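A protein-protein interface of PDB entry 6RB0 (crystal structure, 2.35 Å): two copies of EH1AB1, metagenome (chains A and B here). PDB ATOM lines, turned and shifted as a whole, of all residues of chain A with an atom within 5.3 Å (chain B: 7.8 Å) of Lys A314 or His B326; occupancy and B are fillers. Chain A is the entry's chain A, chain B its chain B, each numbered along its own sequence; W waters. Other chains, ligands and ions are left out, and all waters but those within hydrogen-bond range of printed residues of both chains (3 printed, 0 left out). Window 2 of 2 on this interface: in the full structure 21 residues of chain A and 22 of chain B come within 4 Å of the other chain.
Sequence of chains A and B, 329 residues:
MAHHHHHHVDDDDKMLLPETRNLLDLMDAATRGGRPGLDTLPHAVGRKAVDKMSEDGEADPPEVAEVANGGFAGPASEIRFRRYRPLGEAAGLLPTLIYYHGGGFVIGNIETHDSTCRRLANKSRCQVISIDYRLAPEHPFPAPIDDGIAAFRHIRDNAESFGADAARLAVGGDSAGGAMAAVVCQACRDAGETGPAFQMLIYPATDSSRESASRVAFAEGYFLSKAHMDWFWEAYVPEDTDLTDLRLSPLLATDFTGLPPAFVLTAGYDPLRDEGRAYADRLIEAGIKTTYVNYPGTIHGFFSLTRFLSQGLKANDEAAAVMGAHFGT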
ATOM      1  N   TYR A 295      10.831  -9.006   2.213  1.00  0.00           N
ATOM      2  CA  TYR A 295       9.711  -9.777   2.801  1.00  0.00           C
ATOM      3  C   TYR A 295       8.485  -9.554   1.926  1.00  0.00           C
ATOM      4  O   TYR A 295       7.747  -8.587   2.104  1.00  0.00           O
ATOM      5  CB  TYR A 295       9.485  -9.356   4.254  1.00  0.00           C
ATOM      6  CG  TYR A 295      10.410 -10.027   5.237  1.00  0.00           C
ATOM      7  CD1 TYR A 295      11.739  -9.657   5.340  1.00  0.00           C
ATOM      8  CD2 TYR A 295       9.953 -11.040   6.066  1.00  0.00           C
ATOM      9  CE1 TYR A 295      12.596 -10.284   6.233  1.00  0.00           C
ATOM     10  CE2 TYR A 295      10.798 -11.676   6.964  1.00  0.00           C
ATOM     11  CZ  TYR A 295      12.123 -11.300   7.043  1.00  0.00           C
ATOM     12  OH  TYR A 295      12.957 -11.925   7.920  1.00  0.00           O
ATOM     13  N   SER A 310       3.178 -11.979  12.336  1.00  0.00           N
ATOM     14  CA  SER A 310       4.260 -12.920  12.717  1.00  0.00           C
ATOM     15  C   SER A 310       5.490 -12.727  11.814  1.00  0.00           C
ATOM     16  O   SER A 310       6.612 -12.946  12.308  1.00  0.00           O
ATOM     17  CB  SER A 310       3.757 -14.339  12.681  1.00  0.00           C
ATOM     18  OG  SER A 310       3.314 -14.698  11.378  1.00  0.00           O
ATOM     19  N   GLN A 311       5.306 -12.339  10.547  1.00  0.00           N
ATOM     20  CA  GLN A 311       6.440 -12.032   9.632  1.00  0.00           C
ATOM     21  C   GLN A 311       7.336 -10.973  10.285  1.00  0.00           C
ATOM     22  O   GLN A 311       8.553 -10.991  10.031  1.00  0.00           O
ATOM     23  CB  GLN A 311       5.947 -11.545   8.270  1.00  0.00           C
ATOM     24  CG  GLN A 311       5.396 -12.661   7.407  1.00  0.00           C
ATOM     25  CD  GLN A 311       6.495 -13.603   6.980  1.00  0.00           C
ATOM     26  OE1 GLN A 311       7.389 -13.233   6.232  1.00  0.00           O
ATOM     27  NE2 GLN A 311       6.450 -14.826   7.472  1.00  0.00           N
ATOM     28  N   GLY A 312       6.752 -10.081  11.084  1.00  0.00           N
ATOM     29  CA  GLY A 312       7.498  -9.013  11.771  1.00  0.00           C
ATOM     30  C   GLY A 312       8.456  -9.578  12.800  1.00  0.00           C
ATOM     31  O   GLY A 312       9.574  -9.050  12.931  1.00  0.00           O
ATOM     32  N   LEU A 313       8.032 -10.616  13.515  1.00  0.00           N
ATOM     33  CA  LEU A 313       8.876 -11.309  14.521  1.00  0.00           C
ATOM     34  C   LEU A 313      10.027 -12.000  13.790  1.00  0.00           C
ATOM     35  O   LEU A 313      11.163 -11.947  14.303  1.00  0.00           O
ATOM     36  CB  LEU A 313       8.016 -12.294  15.310  1.00  0.00           C
ATOM     37  CG  LEU A 313       6.944 -11.650  16.187  1.00  0.00           C
ATOM     38  CD1 LEU A 313       6.088 -12.719  16.842  1.00  0.00           C
ATOM     39  CD2 LEU A 313       7.570 -10.739  17.242  1.00  0.00           C
ATOM     40  N   LYS A 314       9.757 -12.550  12.605  1.00  0.00           N
ATOM     41  CA  LYS A 314      10.789 -13.185  11.747  1.00  0.00           C
ATOM     42  C   LYS A 314      11.789 -12.123  11.283  1.00  0.00           C
ATOM     43  O   LYS A 314      13.002 -12.379  11.334  1.00  0.00           O
ATOM     44  CB  LYS A 314      10.128 -13.890  10.564  1.00  0.00           C
ATOM     45  CG  LYS A 314       9.236 -15.052  10.960  1.00  0.00           C
ATOM     46  CD  LYS A 314       9.321 -16.217  10.004  1.00  0.00           C
ATOM     47  CE  LYS A 314       8.774 -17.508  10.583  1.00  0.00           C
ATOM     48  NZ  LYS A 314       9.356 -17.826  11.913  1.00  0.00           N
ATOM     49  N   ALA A 315      11.287 -10.967  10.856  1.00  0.00           N
ATOM     50  CA  ALA A 315      12.106  -9.822  10.416  1.00  0.00           C
ATOM     51  C   ALA A 315      12.941  -9.312  11.594  1.00  0.00           C
ATOM     52  O   ALA A 315      14.147  -9.079  11.394  1.00  0.00           O
ATOM     53  CB  ALA A 315      11.222  -8.744   9.847  1.00  0.00           C
ATOM     54  N   ASN A 316      12.326  -9.159  12.774  1.00  0.00           N
ATOM     55  CA  ASN A 316      13.033  -8.779  14.028  1.00  0.00           C
ATOM     56  C   ASN A 316      14.238  -9.703  14.202  1.00  0.00           C
ATOM     57  O   ASN A 316      15.363  -9.192  14.367  1.00  0.00           O
ATOM     58  CB  ASN A 316      12.154  -8.872  15.280  1.00  0.00           C
ATOM     59  CG  ASN A 316      11.021  -7.870  15.331  1.00  0.00           C
ATOM     60  OD1 ASN A 316      10.134  -8.004  16.170  1.00  0.00           O
ATOM     61  ND2 ASN A 316      11.029  -6.876  14.450  1.00  0.00           N
ATOM     62  N   ASP A 317      14.003 -11.014  14.134  1.00  0.00           N
ATOM     63  CA  ASP A 317      15.022 -12.057  14.425  1.00  0.00           C
ATOM     64  C   ASP A 317      16.101 -12.041  13.335  1.00  0.00           C
ATOM     65  O   ASP A 317      17.281 -12.230  13.660  1.00  0.00           O
ATOM     66  CB  ASP A 317      14.371 -13.429  14.582  1.00  0.00           C
ATOM     67  CG  ASP A 317      13.386 -13.522  15.743  1.00  0.00           C
ATOM     68  OD1 ASP A 317      13.372 -12.605  16.600  1.00  0.00           O
ATOM     69  OD2 ASP A 317      12.604 -14.507  15.760  1.00  0.00           O
ATOM     70  N   GLU A 318      15.723 -11.806  12.084  1.00  0.00           N
ATOM     71  CA  GLU A 318      16.712 -11.734  10.982  1.00  0.00           C
ATOM     72  C   GLU A 318      17.591 -10.492  11.170  1.00  0.00           C
ATOM     73  O   GLU A 318      18.803 -10.635  11.161  1.00  0.00           O
ATOM     74  CB  GLU A 318      16.029 -11.745   9.623  1.00  0.00           C
ATOM     75  CG  GLU A 318      17.046 -11.718   8.500  1.00  0.00           C
ATOM     76  CD  GLU A 318      16.536 -12.030   7.108  1.00  0.00           C
ATOM     77  OE1 GLU A 318      15.297 -12.180   6.933  1.00  0.00           O
ATOM     78  OE2 GLU A 318      17.391 -12.104   6.194  1.00  0.00           O
ATOM     79  N   ALA A 319      17.010  -9.309  11.358  1.00  0.00           N
ATOM     80  CA  ALA A 319      17.792  -8.080  11.614  1.00  0.00           C
ATOM     81  C   ALA A 319      18.753  -8.314  12.792  1.00  0.00           C
ATOM     82  O   ALA A 319      19.954  -8.024  12.644  1.00  0.00           O
ATOM     83  CB  ALA A 319      16.868  -6.914  11.852  1.00  0.00           C
ATOM     84  N   PRO B  95      14.743 -28.401  13.305  1.00  0.00           N
ATOM     85  CA  PRO B  95      14.855 -27.790  11.988  1.00  0.00           C
ATOM     86  C   PRO B  95      16.241 -28.246  11.515  1.00  0.00           C
ATOM     87  O   PRO B  95      17.160 -28.375  12.333  1.00  0.00           O
ATOM     88  CB  PRO B  95      14.723 -26.288  12.267  1.00  0.00           C
ATOM     89  CG  PRO B  95      15.205 -26.153  13.703  1.00  0.00           C
ATOM     90  CD  PRO B  95      14.700 -27.405  14.391  1.00  0.00           C
ATOM     91  N   CYS B 126      20.057 -25.315  14.529  1.00  0.00           N
ATOM     92  CA  CYS B 126      19.485 -26.330  13.610  1.00  0.00           C
ATOM     93  C   CYS B 126      20.437 -27.516  13.530  1.00  0.00           C
ATOM     94  O   CYS B 126      21.653 -27.320  13.681  1.00  0.00           O
ATOM     95  CB  CYS B 126      19.305 -25.810  12.189  1.00  0.00           C
ATOM     96  SG  CYS B 126      18.149 -24.427  12.064  1.00  0.00           S
ATOM     97  N   ALA B 167       8.665 -30.081   8.516  1.00  0.00           N
ATOM     98  CA  ALA B 167       8.161 -28.718   8.215  1.00  0.00           C
ATOM     99  C   ALA B 167       9.324 -27.722   8.063  1.00  0.00           C
ATOM    100  O   ALA B 167       9.064 -26.598   7.567  1.00  0.00           O
ATOM    101  CB  ALA B 167       7.191 -28.267   9.279  1.00  0.00           C
ATOM    102  N   ARG B 168      10.543 -28.084   8.490  1.00  0.00           N
ATOM    103  CA  ARG B 168      11.697 -27.136   8.545  1.00  0.00           C
ATOM    104  C   ARG B 168      12.962 -27.851   8.056  1.00  0.00           C
ATOM    105  O   ARG B 168      13.947 -28.004   8.828  1.00  0.00           O
ATOM    106  CB  ARG B 168      11.791 -26.536   9.950  1.00  0.00           C
ATOM    107  CG  ARG B 168      10.623 -25.616  10.274  1.00  0.00           C
ATOM    108  CD  ARG B 168      10.740 -24.975  11.636  1.00  0.00           C
ATOM    109  NE  ARG B 168      10.794 -26.001  12.666  1.00  0.00           N
ATOM    110  CZ  ARG B 168      11.250 -25.827  13.906  1.00  0.00           C
ATOM    111  NH1 ARG B 168      11.720 -24.653  14.300  1.00  0.00           N
ATOM    112  NH2 ARG B 168      11.239 -26.850  14.743  1.00  0.00           N
ATOM    113  N   ALA B 170      15.840 -27.515   5.312  1.00  0.00           N
ATOM    114  CA  ALA B 170      16.578 -26.627   4.398  1.00  0.00           C
ATOM    115  C   ALA B 170      17.588 -27.462   3.616  1.00  0.00           C
ATOM    116  O   ALA B 170      17.989 -28.548   4.092  1.00  0.00           O
ATOM    117  CB  ALA B 170      17.253 -25.532   5.176  1.00  0.00           C
ATOM    118  N   PRO B 196      12.343 -28.217  -0.342  1.00  0.00           N
ATOM    119  CA  PRO B 196      12.915 -27.690   0.895  1.00  0.00           C
ATOM    120  C   PRO B 196      12.142 -26.456   1.382  1.00  0.00           C
ATOM    121  O   PRO B 196      11.537 -25.778   0.578  1.00  0.00           O
ATOM    122  CB  PRO B 196      14.353 -27.332   0.502  1.00  0.00           C
ATOM    123  CG  PRO B 196      14.613 -28.177  -0.719  1.00  0.00           C
ATOM    124  CD  PRO B 196      13.294 -28.146  -1.462  1.00  0.00           C
ATOM    125  N   ALA B 197      12.154 -26.219   2.691  1.00  0.00           N
ATOM    126  CA  ALA B 197      11.532 -25.035   3.330  1.00  0.00           C
ATOM    127  C   ALA B 197      12.429 -23.816   3.118  1.00  0.00           C
ATOM    128  O   ALA B 197      11.943 -22.679   3.293  1.00  0.00           O
ATOM    129  CB  ALA B 197      11.310 -25.281   4.797  1.00  0.00           C
ATOM    130  N   PHE B 198      13.696 -24.041   2.768  1.00  0.00           N
ATOM    131  CA  PHE B 198      14.728 -22.980   2.774  1.00  0.00           C
ATOM    132  C   PHE B 198      15.941 -23.438   1.975  1.00  0.00           C
ATOM    133  O   PHE B 198      16.268 -24.648   1.994  1.00  0.00           O
ATOM    134  CB  PHE B 198      15.090 -22.624   4.219  1.00  0.00           C
ATOM    135  CG  PHE B 198      15.962 -21.403   4.369  1.00  0.00           C
ATOM    136  CD1 PHE B 198      17.345 -21.516   4.435  1.00  0.00           C
ATOM    137  CD2 PHE B 198      15.403 -20.138   4.430  1.00  0.00           C
ATOM    138  CE1 PHE B 198      18.144 -20.391   4.568  1.00  0.00           C
ATOM    139  CE2 PHE B 198      16.204 -19.014   4.570  1.00  0.00           C
ATOM    140  CZ  PHE B 198      17.571 -19.144   4.642  1.00  0.00           C
ATOM    141  N   GLN B 199      16.600 -22.488   1.313  1.00  0.00           N
ATOM    142  CA  GLN B 199      17.810 -22.765   0.498  1.00  0.00           C
ATOM    143  C   GLN B 199      18.902 -21.760   0.879  1.00  0.00           C
ATOM    144  O   GLN B 199      18.668 -20.535   0.764  1.00  0.00           O
ATOM    145  CB  GLN B 199      17.475 -22.804  -0.993  1.00  0.00           C
ATOM    146  CG  GLN B 199      16.972 -21.492  -1.578  1.00  0.00           C
ATOM    147  CD  GLN B 199      16.656 -21.618  -3.051  1.00  0.00           C
ATOM    148  OE1 GLN B 199      17.444 -22.168  -3.827  1.00  0.00           O
ATOM    149  NE2 GLN B 199      15.499 -21.100  -3.450  1.00  0.00           N
ATOM    150  N   PRO B 260      11.668 -22.046  -2.645  1.00  0.00           N
ATOM    151  CA  PRO B 260      11.640 -21.733  -1.225  1.00  0.00           C
ATOM    152  C   PRO B 260      12.428 -20.470  -0.895  1.00  0.00           C
ATOM    153  O   PRO B 260      13.310 -20.050  -1.645  1.00  0.00           O
ATOM    154  CB  PRO B 260      12.243 -22.973  -0.549  1.00  0.00           C
ATOM    155  CG  PRO B 260      13.121 -23.575  -1.618  1.00  0.00           C
ATOM    156  CD  PRO B 260      12.492 -23.221  -2.951  1.00  0.00           C
ATOM    157  N   PRO B 261      12.104 -19.845   0.257  1.00  0.00           N
ATOM    158  CA  PRO B 261      12.852 -18.707   0.779  1.00  0.00           C
ATOM    159  C   PRO B 261      14.356 -18.991   0.808  1.00  0.00           C
ATOM    160  O   PRO B 261      14.747 -20.116   1.082  1.00  0.00           O
ATOM    161  CB  PRO B 261      12.295 -18.554   2.197  1.00  0.00           C
ATOM    162  CG  PRO B 261      10.871 -19.051   2.068  1.00  0.00           C
ATOM    163  CD  PRO B 261      10.990 -20.234   1.136  1.00  0.00           C
ATOM    164  N   ALA B 262      15.161 -17.975   0.521  1.00  0.00           N
ATOM    165  CA  ALA B 262      16.583 -18.173   0.174  1.00  0.00           C
ATOM    166  C   ALA B 262      17.470 -17.194   0.927  1.00  0.00           C
ATOM    167  O   ALA B 262      17.052 -16.067   1.192  1.00  0.00           O
ATOM    168  CB  ALA B 262      16.788 -18.032  -1.313  1.00  0.00           C
ATOM    169  N   LYS B 289      10.840 -14.719  -0.692  1.00  0.00           N
ATOM    170  CA  LYS B 289      11.545 -14.104   0.458  1.00  0.00           C
ATOM    171  C   LYS B 289      13.026 -14.443   0.295  1.00  0.00           C
ATOM    172  O   LYS B 289      13.357 -15.640   0.254  1.00  0.00           O
ATOM    173  CB  LYS B 289      10.961 -14.594   1.785  1.00  0.00           C
ATOM    174  CG  LYS B 289      11.446 -13.845   3.015  1.00  0.00           C
ATOM    175  CD  LYS B 289      12.354 -14.646   3.918  1.00  0.00           C
ATOM    176  CE  LYS B 289      13.374 -13.766   4.612  1.00  0.00           C
ATOM    177  NZ  LYS B 289      14.112 -14.493   5.675  1.00  0.00           N
ATOM    178  N   THR B 291      17.225 -13.219   1.117  1.00  0.00           N
ATOM    179  CA  THR B 291      18.336 -12.457   1.724  1.00  0.00           C
ATOM    180  C   THR B 291      19.542 -12.605   0.801  1.00  0.00           C
ATOM    181  O   THR B 291      19.910 -13.758   0.489  1.00  0.00           O
ATOM    182  CB  THR B 291      18.620 -12.936   3.151  1.00  0.00           C
ATOM    183  OG1 THR B 291      17.383 -12.886   3.857  1.00  0.00           O
ATOM    184  CG2 THR B 291      19.666 -12.091   3.843  1.00  0.00           C
ATOM    185  N   ALA B 320      23.976 -18.951   9.271  1.00  0.00           N
ATOM    186  CA  ALA B 320      23.350 -19.717  10.376  1.00  0.00           C
ATOM    187  C   ALA B 320      22.228 -18.904  11.027  1.00  0.00           C
ATOM    188  O   ALA B 320      21.135 -19.438  11.251  1.00  0.00           O
ATOM    189  CB  ALA B 320      24.389 -20.085  11.401  1.00  0.00           C
ATOM    190  N   ALA B 321      22.503 -17.640  11.321  1.00  0.00           N
ATOM    191  CA  ALA B 321      21.580 -16.753  12.054  1.00  0.00           C
ATOM    192  C   ALA B 321      20.334 -16.488  11.200  1.00  0.00           C
ATOM    193  O   ALA B 321      19.209 -16.505  11.757  1.00  0.00           O
ATOM    194  CB  ALA B 321      22.305 -15.490  12.436  1.00  0.00           C
ATOM    195  N   VAL B 322      20.510 -16.268   9.898  1.00  0.00           N
ATOM    196  CA  VAL B 322      19.372 -16.013   8.962  1.00  0.00           C
ATOM    197  C   VAL B 322      18.510 -17.272   8.844  1.00  0.00           C
ATOM    198  O   VAL B 322      17.265 -17.146   8.844  1.00  0.00           O
ATOM    199  CB  VAL B 322      19.851 -15.548   7.579  1.00  0.00           C
ATOM    200  CG1 VAL B 322      18.724 -15.566   6.553  1.00  0.00           C
ATOM    201  CG2 VAL B 322      20.483 -14.174   7.672  1.00  0.00           C
ATOM    202  N   MET B 323      19.130 -18.443   8.711  1.00  0.00           N
ATOM    203  CA  MET B 323      18.356 -19.701   8.626  1.00  0.00           C
ATOM    204  C   MET B 323      17.617 -19.909   9.960  1.00  0.00           C
ATOM    205  O   MET B 323      16.405 -20.169   9.929  1.00  0.00           O
ATOM    206  CB  MET B 323      19.258 -20.895   8.327  1.00  0.00           C
ATOM    207  CG  MET B 323      18.470 -22.174   8.161  1.00  0.00           C
ATOM    208  SD  MET B 323      19.525 -23.538   7.679  1.00  0.00           S
ATOM    209  CE  MET B 323      20.662 -23.613   9.067  1.00  0.00           C
ATOM    210  N   GLY B 324      18.327 -19.765  11.078  1.00  0.00           N
ATOM    211  CA  GLY B 324      17.763 -19.856  12.434  1.00  0.00           C
ATOM    212  C   GLY B 324      16.561 -18.938  12.591  1.00  0.00           C
ATOM    213  O   GLY B 324      15.543 -19.382  13.152  1.00  0.00           O
ATOM    214  N   ALA B 325      16.649 -17.707  12.087  1.00  0.00           N
ATOM    215  CA  ALA B 325      15.565 -16.712  12.224  1.00  0.00           C
ATOM    216  C   ALA B 325      14.361 -17.177  11.402  1.00  0.00           C
ATOM    217  O   ALA B 325      13.221 -17.054  11.880  1.00  0.00           O
ATOM    218  CB  ALA B 325      16.028 -15.346  11.798  1.00  0.00           C
ATOM    219  N   HIS B 326      14.598 -17.702  10.203  1.00  0.00           N
ATOM    220  CA  HIS B 326      13.507 -18.152   9.307  1.00  0.00           C
ATOM    221  C   HIS B 326      12.739 -19.291   9.988  1.00  0.00           C
ATOM    222  O   HIS B 326      11.512 -19.354   9.858  1.00  0.00           O
ATOM    223  CB  HIS B 326      14.059 -18.566   7.950  1.00  0.00           C
ATOM    224  CG  HIS B 326      12.977 -18.984   7.021  1.00  0.00           C
ATOM    225  ND1 HIS B 326      12.199 -18.060   6.338  1.00  0.00           N
ATOM    226  CD2 HIS B 326      12.512 -20.211   6.699  1.00  0.00           C
ATOM    227  CE1 HIS B 326      11.314 -18.713   5.609  1.00  0.00           C
ATOM    228  NE2 HIS B 326      11.484 -20.037   5.814  1.00  0.00           N
ATOM    229  N   PHE B 327      13.458 -20.135  10.719  1.00  0.00           N
ATOM    230  CA  PHE B 327      12.921 -21.354  11.366  1.00  0.00           C
ATOM    231  C   PHE B 327      12.489 -21.076  12.811  1.00  0.00           C
ATOM    232  O   PHE B 327      12.017 -22.017  13.454  1.00  0.00           O
ATOM    233  CB  PHE B 327      13.963 -22.468  11.280  1.00  0.00           C
ATOM    234  CG  PHE B 327      14.066 -23.124   9.929  1.00  0.00           C
ATOM    235  CD1 PHE B 327      13.010 -23.099   9.034  1.00  0.00           C
ATOM    236  CD2 PHE B 327      15.216 -23.807   9.569  1.00  0.00           C
ATOM    237  CE1 PHE B 327      13.109 -23.734   7.805  1.00  0.00           C
ATOM    238  CE2 PHE B 327      15.306 -24.453   8.341  1.00  0.00           C
ATOM    239  CZ  PHE B 327      14.258 -24.407   7.457  1.00  0.00           C
ATOM    240  N   GLY B 328      12.617 -19.837  13.291  1.00  0.00           N
ATOM    241  CA  GLY B 328      12.200 -19.446  14.651  1.00  0.00           C
ATOM    242  C   GLY B 328      12.938 -20.236  15.719  1.00  0.00           C
ATOM    243  O   GLY B 328      12.307 -20.613  16.719  1.00  0.00           O
ATOM    244  N   THR B 329      14.233 -20.484  15.531  1.00  0.00           N
ATOM    245  CA  THR B 329      15.082 -21.176  16.540  1.00  0.00           C
ATOM    246  C   THR B 329      15.538 -20.153  17.590  1.00  0.00           C
ATOM    247  O   THR B 329      15.288 -18.953  17.457  1.00  0.00           O
ATOM    248  CB  THR B 329      16.267 -21.907  15.896  1.00  0.00           C
ATOM    249  OG1 THR B 329      17.207 -20.911  15.489  1.00  0.00           O
ATOM    250  CG2 THR B 329      15.858 -22.785  14.731  1.00  0.00           C
ATOM    251  OXT THR B 329      16.173 -20.488  18.602  1.00  0.00           O
HETATM  252  O   HOH W   1      12.049 -16.151  13.934  1.00  0.00           O
HETATM  253  O   HOH W   2      15.659 -15.361   7.864  1.00  0.00           O
HETATM  254  O   HOH W   3      13.331 -14.595   9.426  1.00  0.00           O
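The side-chain carboxylate (OE1) of Glu A318 lies within salt-bridge range of the side-chain amino group (NZ) of Lys B289, 2.9 Å away.
The side-chain carboxylate (OE2) of Glu A318 lies within hydrogen-bond range of the side-chain hydroxyl (OG1) of Thr B291, 2.5 Å away.
The side-chain amino group of Lys A314 is in hydrogen-bond range of the backbone carbonyl oxygen of His B326, at 3.3 Å.
N of Ala B262 lies within hydrogen-bond range of O of Lys B289, 3.0 Å away.
OH of Tyr A295 is in hydrogen-bond range of OE1 of Glu A318 (2.6 Å).
OH of Tyr A295 lies within hydrogen-bond range of O of Lys A314, 3.4 Å away.
The backbone carbonyl oxygen (O) of Ala B262 lies within hydrogen-bond range of the backbone NH (N) of Thr B291, at 2.9 Å.
No position is printed for both chains.
Of the 8 pairs that touch across the chains among the printed residues, none has its exchanged pair printed and touching as well.
Lys A314 touches just these residues of chain B: Ala B325 and His B326.
His B326 touches just one residue of chain A: Lys A314.
No residue of chain B comes within 4 Å of Ala A315.
Printed residues of chain B within 4 Å of Glu A318: Lys B289 (2.9 Å), Thr B291 (2.5 Å), Val B322 (3.7 Å) and Ala B325 (3.6 Å).
Of the printed residues of chain A, Val B322 touches Glu A318.
Printed residues of chain B within 4 Å of Asp A317: Ala B325 (3.6 Å).
Ala B170 touches none of the printed residues of chain A.
The nearest printed residue of chain A that does not touch Lys B289 is Gln A311 (5.2 Å).
Tyr A295 touches Lys B289.
Ala B325 touches Lys A314.
Asp A317 touches Ala B325 (C to CB, 3.6 Å).
Val B322 touches Glu A318 (CG1 to OE2, 3.7 Å).
Glu A318 touches Ala B325.
Of the 24 printed residues of chain B, 5 touch a printed residue of chain A.
Printed residues of chain B that touch a printed residue of chain A: Lys B289, Thr B291, Val B322, Ala B325 and His B326.
Printed residues of chain A that touch a printed residue of chain B: Tyr A295, Lys A314, Asp A317 and Glu A318.
Among the printed residues, 8 pairs touch across the chains.
Water W1 lies within hydrogen-bond range of the side-chain carboxylate of Asp A317 and the backbone carbonyl oxygen of Ala B325.
Water W2 lies within hydrogen-bond range of O of Val B322 (2.6 Å), NZ of Lys B289 (2.8 Å), OE1 of Glu A318 (3.3 Å) and N of His B326 (3.5 Å).
Water W3 lies within hydrogen-bond range of the backbone carbonyl oxygen of Lys A314 (2.9 Å), the side-chain hydroxyl of Tyr A295 (3.1 Å), the backbone NH of His B326 (3.4 Å) and the backbone carbonyl oxygen of Ala B325 (3.5 Å).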
